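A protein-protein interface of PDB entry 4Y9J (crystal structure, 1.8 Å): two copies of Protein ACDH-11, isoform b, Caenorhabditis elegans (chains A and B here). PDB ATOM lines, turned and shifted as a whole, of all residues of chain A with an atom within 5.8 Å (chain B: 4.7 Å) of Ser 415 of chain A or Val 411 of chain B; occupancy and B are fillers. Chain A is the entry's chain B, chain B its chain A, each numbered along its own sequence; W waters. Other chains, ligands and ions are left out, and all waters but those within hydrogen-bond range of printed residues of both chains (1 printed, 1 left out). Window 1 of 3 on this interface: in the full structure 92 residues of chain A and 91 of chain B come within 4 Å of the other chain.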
ATOM      1  N   ALA A 410       8.075  14.959 -26.979  1.00  0.00           N
ATOM      2  CA  ALA A 410       8.716  14.242 -25.869  1.00  0.00           C
ATOM      3  C   ALA A 410       8.920  15.131 -24.615  1.00  0.00           C
ATOM      4  O   ALA A 410       8.527  14.726 -23.543  1.00  0.00           O
ATOM      5  CB  ALA A 410      10.059  13.664 -26.286  1.00  0.00           C
ATOM      6  N   VAL A 411       9.493  16.319 -24.758  1.00  0.00           N
ATOM      7  CA  VAL A 411       9.760  17.111 -23.565  1.00  0.00           C
ATOM      8  C   VAL A 411       8.479  17.583 -22.876  1.00  0.00           C
ATOM      9  O   VAL A 411       8.342  17.385 -21.701  1.00  0.00           O
ATOM     10  CB  VAL A 411      10.743  18.262 -23.789  1.00  0.00           C
ATOM     11  CG1 VAL A 411      10.857  19.151 -22.545  1.00  0.00           C
ATOM     12  CG2 VAL A 411      12.146  17.707 -24.142  1.00  0.00           C
ATOM     13  N   PRO A 412       7.513  18.154 -23.611  1.00  0.00           N
ATOM     14  CA  PRO A 412       6.311  18.494 -22.850  1.00  0.00           C
ATOM     15  C   PRO A 412       5.588  17.309 -22.221  1.00  0.00           C
ATOM     16  O   PRO A 412       5.002  17.494 -21.147  1.00  0.00           O
ATOM     17  CB  PRO A 412       5.391  19.141 -23.881  1.00  0.00           C
ATOM     18  CG  PRO A 412       6.345  19.652 -24.940  1.00  0.00           C
ATOM     19  CD  PRO A 412       7.475  18.663 -24.994  1.00  0.00           C
ATOM     20  N   MET A 413       5.573  16.159 -22.891  1.00  0.00           N
ATOM     21  CA  MET A 413       4.925  15.008 -22.302  1.00  0.00           C
ATOM     22  C   MET A 413       5.712  14.484 -21.058  1.00  0.00           C
ATOM     23  O   MET A 413       5.108  14.160 -20.040  1.00  0.00           O
ATOM     24  CB  MET A 413       4.771  13.869 -23.297  1.00  0.00           C
ATOM     25  CG  MET A 413       3.720  12.878 -22.778  1.00  0.00           C
ATOM     26  SD  MET A 413       3.427  11.546 -23.887  1.00  0.00           S
ATOM     27  CE  MET A 413       2.526  12.520 -25.125  1.00  0.00           C
ATOM     28  N   VAL A 414       7.019  14.407 -21.117  1.00  0.00           N
ATOM     29  CA  VAL A 414       7.765  13.906 -19.969  1.00  0.00           C
ATOM     30  C   VAL A 414       7.692  14.954 -18.833  1.00  0.00           C
ATOM     31  O   VAL A 414       7.546  14.562 -17.695  1.00  0.00           O
ATOM     32  CB  VAL A 414       9.217  13.580 -20.304  1.00  0.00           C
ATOM     33  CG1 VAL A 414       9.994  13.159 -19.061  1.00  0.00           C
ATOM     34  CG2 VAL A 414       9.232  12.456 -21.305  1.00  0.00           C
ATOM     35  N   SER A 415       7.661  16.252 -19.188  1.00  0.00           N
ATOM     36  CA  SER A 415       7.477  17.299 -18.173  1.00  0.00           C
ATOM     37  C   SER A 415       6.146  17.088 -17.402  1.00  0.00           C
ATOM     38  O   SER A 415       6.098  17.275 -16.187  1.00  0.00           O
ATOM     39  CB  SER A 415       7.583  18.688 -18.801  1.00  0.00           C
ATOM     40  OG  SER A 415       7.361  19.712 -17.862  1.00  0.00           O
ATOM     41  N   GLU A 416       5.063  16.850 -18.130  1.00  0.00           N
ATOM     42  CA  GLU A 416       3.753  16.552 -17.547  1.00  0.00           C
ATOM     43  C   GLU A 416       3.820  15.328 -16.664  1.00  0.00           C
ATOM     44  O   GLU A 416       3.267  15.281 -15.566  1.00  0.00           O
ATOM     45  CB  GLU A 416       2.655  16.374 -18.642  1.00  0.00           C
ATOM     46  CG  GLU A 416       1.232  16.462 -18.109  1.00  0.00           C
ATOM     47  CD  GLU A 416       0.921  17.822 -17.546  1.00  0.00           C
ATOM     48  OE1 GLU A 416       1.011  18.815 -18.337  1.00  0.00           O
ATOM     49  OE2 GLU A 416       0.580  17.917 -16.326  1.00  0.00           O
ATOM     50  N   GLY A 417       4.547  14.336 -17.121  1.00  0.00           N
ATOM     51  CA  GLY A 417       4.703  13.098 -16.360  1.00  0.00           C
ATOM     52  C   GLY A 417       5.426  13.249 -15.057  1.00  0.00           C
ATOM     53  O   GLY A 417       4.970  12.693 -14.016  1.00  0.00           O
ATOM     54  N   ILE A 418       6.497  14.004 -15.052  1.00  0.00           N
ATOM     55  CA  ILE A 418       7.217  14.199 -13.806  1.00  0.00           C
ATOM     56  C   ILE A 418       6.380  14.958 -12.797  1.00  0.00           C
ATOM     57  O   ILE A 418       6.402  14.630 -11.636  1.00  0.00           O
ATOM     58  CB  ILE A 418       8.644  14.762 -13.902  1.00  0.00           C
ATOM     59  CG1 ILE A 418       8.675  16.114 -14.409  1.00  0.00           C
ATOM     60  CG2 ILE A 418       9.685  13.835 -14.690  1.00  0.00           C
ATOM     61  CD1 ILE A 418       9.966  16.776 -13.995  1.00  0.00           C
ATOM     62  N   GLU A 419       5.505  15.851 -13.257  1.00  0.00           N
ATOM     63  CA  GLU A 419       4.620  16.594 -12.373  1.00  0.00           C
ATOM     64  C   GLU A 419       3.580  15.693 -11.701  1.00  0.00           C
ATOM     65  O   GLU A 419       3.136  16.028 -10.626  1.00  0.00           O
ATOM     66  CB  GLU A 419       3.948  17.722 -13.186  1.00  0.00           C
ATOM     67  CG  GLU A 419       2.975  18.632 -12.438  1.00  0.00           C
ATOM     68  CD  GLU A 419       2.487  19.784 -13.331  1.00  0.00           C
ATOM     69  OE1 GLU A 419       3.269  20.162 -14.246  1.00  0.00           O
ATOM     70  OE2 GLU A 419       1.328  20.250 -13.157  1.00  0.00           O
ATOM     71  N   CYS A 420       3.223  14.545 -12.291  1.00  0.00           N
ATOM     72  CA  CYS A 420       2.368  13.604 -11.628  1.00  0.00           C
ATOM     73  C   CYS A 420       2.953  13.139 -10.276  1.00  0.00           C
ATOM     74  O   CYS A 420       2.214  12.638  -9.432  1.00  0.00           O
ATOM     75  CB  CYS A 420       2.117  12.351 -12.447  1.00  0.00           C
ATOM     76  SG  CYS A 420       1.269  12.664 -14.030  1.00  0.00           S
ATOM     77  N   LEU A 436      13.544  13.326 -18.204  1.00  0.00           N
ATOM     78  CA  LEU A 436      13.288  14.630 -18.835  1.00  0.00           C
ATOM     79  C   LEU A 436      14.565  15.200 -19.506  1.00  0.00           C
ATOM     80  O   LEU A 436      14.541  15.650 -20.677  1.00  0.00           O
ATOM     81  CB  LEU A 436      12.803  15.645 -17.814  1.00  0.00           C
ATOM     82  CG  LEU A 436      12.496  17.026 -18.315  1.00  0.00           C
ATOM     83  CD1 LEU A 436      11.299  17.058 -19.234  1.00  0.00           C
ATOM     84  CD2 LEU A 436      12.276  17.939 -17.140  1.00  0.00           C
ATOM     85  N   GLY B 407       2.890  28.713 -15.510  1.00  0.00           N
ATOM     86  CA  GLY B 407       3.672  27.560 -15.052  1.00  0.00           C
ATOM     87  C   GLY B 407       3.692  26.485 -16.122  1.00  0.00           C
ATOM     88  O   GLY B 407       4.715  25.793 -16.269  1.00  0.00           O
ATOM     89  N   LYS B 408       2.536  26.266 -16.769  1.00  0.00           N
ATOM     90  CA  LYS B 408       2.404  25.212 -17.789  1.00  0.00           C
ATOM     91  C   LYS B 408       2.989  25.634 -19.161  1.00  0.00           C
ATOM     92  O   LYS B 408       3.395  24.788 -19.918  1.00  0.00           O
ATOM     93  CB  LYS B 408       1.003  24.699 -17.865  1.00  0.00           C
ATOM     94  CG  LYS B 408       0.793  23.495 -18.787  1.00  0.00           C
ATOM     95  CD  LYS B 408       1.837  22.384 -18.559  1.00  0.00           C
ATOM     96  CE  LYS B 408       1.842  21.908 -17.122  1.00  0.00           C
ATOM     97  NZ  LYS B 408       2.695  20.678 -16.927  1.00  0.00           N
ATOM     98  N   GLN B 409       3.006  26.924 -19.495  1.00  0.00           N
ATOM     99  CA  GLN B 409       3.721  27.440 -20.641  1.00  0.00           C
ATOM    100  C   GLN B 409       5.236  27.270 -20.554  1.00  0.00           C
ATOM    101  O   GLN B 409       5.873  27.108 -21.561  1.00  0.00           O
ATOM    102  CB  GLN B 409       3.467  28.904 -20.852  1.00  0.00           C
ATOM    103  CG  GLN B 409       2.045  29.252 -21.236  1.00  0.00           C
ATOM    104  CD  GLN B 409       1.915  30.757 -21.355  1.00  0.00           C
ATOM    105  OE1 GLN B 409       2.133  31.500 -20.373  1.00  0.00           O
ATOM    106  NE2 GLN B 409       1.650  31.215 -22.549  1.00  0.00           N
ATOM    107  N   ALA B 410       5.798  27.367 -19.356  1.00  0.00           N
ATOM    108  CA  ALA B 410       7.196  27.643 -19.194  1.00  0.00           C
ATOM    109  C   ALA B 410       8.122  26.560 -19.755  1.00  0.00           C
ATOM    110  O   ALA B 410       9.022  26.875 -20.502  1.00  0.00           O
ATOM    111  CB  ALA B 410       7.528  27.862 -17.706  1.00  0.00           C
ATOM    112  N   VAL B 411       7.924  25.292 -19.381  1.00  0.00           N
ATOM    113  CA  VAL B 411       8.873  24.267 -19.865  1.00  0.00           C
ATOM    114  C   VAL B 411       8.815  24.061 -21.364  1.00  0.00           C
ATOM    115  O   VAL B 411       9.865  24.118 -21.995  1.00  0.00           O
ATOM    116  CB  VAL B 411       8.740  22.941 -19.077  1.00  0.00           C
ATOM    117  CG1 VAL B 411       9.602  21.871 -19.757  1.00  0.00           C
ATOM    118  CG2 VAL B 411       9.197  23.207 -17.637  1.00  0.00           C
ATOM    119  N   PRO B 412       7.599  23.932 -21.956  1.00  0.00           N
ATOM    120  CA  PRO B 412       7.631  23.769 -23.424  1.00  0.00           C
ATOM    121  C   PRO B 412       8.258  24.990 -24.136  1.00  0.00           C
ATOM    122  O   PRO B 412       8.971  24.789 -25.129  1.00  0.00           O
ATOM    123  CB  PRO B 412       6.144  23.582 -23.816  1.00  0.00           C
ATOM    124  CG  PRO B 412       5.547  22.962 -22.558  1.00  0.00           C
ATOM    125  CD  PRO B 412       6.278  23.595 -21.391  1.00  0.00           C
ATOM    126  N   MET B 413       8.023  26.195 -23.647  1.00  0.00           N
ATOM    127  CA  MET B 413       8.611  27.372 -24.285  1.00  0.00           C
ATOM    128  C   MET B 413      10.120  27.429 -24.124  1.00  0.00           C
ATOM    129  O   MET B 413      10.808  27.711 -25.089  1.00  0.00           O
ATOM    130  CB  MET B 413       7.990  28.704 -23.825  1.00  0.00           C
ATOM    131  CG  MET B 413       8.143  29.817 -24.938  1.00  0.00           C
ATOM    132  SD  MET B 413       7.575  31.311 -24.241  1.00  0.00           S
ATOM    133  CE  MET B 413       5.831  30.891 -24.609  1.00  0.00           C
ATOM    134  N   VAL B 414      10.619  27.210 -22.904  1.00  0.00           N
ATOM    135  CA  VAL B 414      12.057  27.221 -22.678  1.00  0.00           C
ATOM    136  C   VAL B 414      12.727  26.106 -23.494  1.00  0.00           C
ATOM    137  O   VAL B 414      13.828  26.298 -24.009  1.00  0.00           O
ATOM    138  CB  VAL B 414      12.466  27.199 -21.156  1.00  0.00           C
ATOM    139  CG1 VAL B 414      13.974  27.211 -21.010  1.00  0.00           C
ATOM    140  CG2 VAL B 414      11.917  28.463 -20.507  1.00  0.00           C
ATOM    141  N   SER B 415      12.081  24.929 -23.552  1.00  0.00           N
ATOM    142  CA  SER B 415      12.565  23.815 -24.328  1.00  0.00           C
ATOM    143  C   SER B 415      12.741  24.221 -25.830  1.00  0.00           C
ATOM    144  O   SER B 415      13.750  23.945 -26.477  1.00  0.00           O
ATOM    145  CB  SER B 415      11.630  22.621 -24.191  1.00  0.00           C
ATOM    146  OG  SER B 415      12.083  21.564 -24.980  1.00  0.00           O
ATOM    147  N   LEU B 436      15.970  25.929 -18.360  1.00  0.00           N
ATOM    148  CA  LEU B 436      15.020  24.866 -18.479  1.00  0.00           C
ATOM    149  C   LEU B 436      14.826  24.112 -17.158  1.00  0.00           C
ATOM    150  O   LEU B 436      13.671  23.887 -16.725  1.00  0.00           O
ATOM    151  CB  LEU B 436      15.490  23.897 -19.556  1.00  0.00           C
ATOM    152  CG  LEU B 436      14.593  22.694 -19.804  1.00  0.00           C
ATOM    153  CD1 LEU B 436      13.314  23.177 -20.458  1.00  0.00           C
ATOM    154  CD2 LEU B 436      15.180  21.666 -20.716  1.00  0.00           C
ATOM    155  N   ALA B 439      13.056  26.483 -14.717  1.00  0.00           N
ATOM    156  CA  ALA B 439      11.666  26.692 -15.111  1.00  0.00           C
ATOM    157  C   ALA B 439      10.790  25.507 -14.754  1.00  0.00           C
ATOM    158  O   ALA B 439       9.617  25.661 -14.471  1.00  0.00           O
ATOM    159  CB  ALA B 439      11.630  26.925 -16.603  1.00  0.00           C
ATOM    160  N   GLN B 440      11.354  24.299 -14.722  1.00  0.00           N
ATOM    161  CA  GLN B 440      10.587  23.104 -14.435  1.00  0.00           C
ATOM    162  C   GLN B 440      10.116  23.061 -12.984  1.00  0.00           C
ATOM    163  O   GLN B 440       9.179  22.361 -12.686  1.00  0.00           O
ATOM    164  CB  GLN B 440      11.412  21.840 -14.836  1.00  0.00           C
ATOM    165  CG  GLN B 440      10.762  20.559 -14.494  1.00  0.00           C
ATOM    166  CD  GLN B 440       9.431  20.278 -15.213  1.00  0.00           C
ATOM    167  OE1 GLN B 440       8.292  20.561 -14.669  1.00  0.00           O
ATOM    168  NE2 GLN B 440       9.531  19.759 -16.379  1.00  0.00           N
HETATM  169  O   HOH W   1       5.150  21.291 -18.126  1.00  0.00           O
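The side-chain amino group of Lys 408 of chain B is in salt-bridge range of the side-chain carboxylate of Glu 416 of chain A (2.9 Å).
The side-chain carboxylate (OE1) of Glu 419 of chain A lies within salt-bridge range of the side-chain amino group (NZ) of Lys 408 of chain B, 2.8 Å away.
NE2 of Gln 440 of chain B is in hydrogen-bond range of OG of Ser 415 of chain A, at 2.6 Å.
The backbone carbonyl oxygen (O) of Glu 416 of chain A lies within hydrogen-bond range of the side-chain sulfur (SG) of Cys 420 of chain A (3.6 Å).
OG of Ser 415 of chain B touches CG1 of Val 411 of chain A (3.6 Å).
Ser 415 of chain A touches Val 411 of chain B (OG to CG1, 3.6 Å).
Gln 440 of chain B touches Ile 418 of chain A.
Leu 436 of chain A touches Gln 440 of chain B (CD2 to NE2, 3.4 Å).
Of chain A, only Ser 415 comes within 4 Å of Val 411 of chain B.
Printed residues of chain B within 4 Å of Leu 436 of chain A: Gln 440.
Of the printed residues of chain B, Glu 419 of chain A touches Lys 408.
Pro 412 of chain B touches none of the printed residues of chain A.
The nearest printed residue of chain B that does not touch Ser 415 of chain A is Lys 408 of chain B (4.9 Å).
The nearest residue of chain A that does not touch Val 411 of chain B is Val 411 of chain A (4.1 Å).
Of the 12 printed residues of chain A, 6 touch a printed residue of chain B.
Hydrophobic or aromatic side chains of chain A within 4 Å of the printed part of chain B: Val 411, Ile 418 and Leu 436.
Printed residues of chain B that touch a printed residue of chain A: Lys 408, Val 411, Ser 415 and Gln 440.
Hydrophobic or aromatic side chains of chain B within 4 Å of the printed part of chain A: Val 411.
Among the printed residues, 7 pairs touch across the chains.
Val 411 of chain A touches Ser 415 of chain B, and with the chains exchanged Ser 415 of chain A touches Val 411 of chain B.
Positions printed for both chains: 410, 411, 412, 413, 414, 415 and 436.
Of the 7 pairs that touch across the chains among the printed residues, 2 have their exchanged pair printed and touching as well.
Water W1 lies within hydrogen-bond range of the side-chain hydroxyl of Ser 415 of chain A and the side-chain amino group of Lys 408 of chain B.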
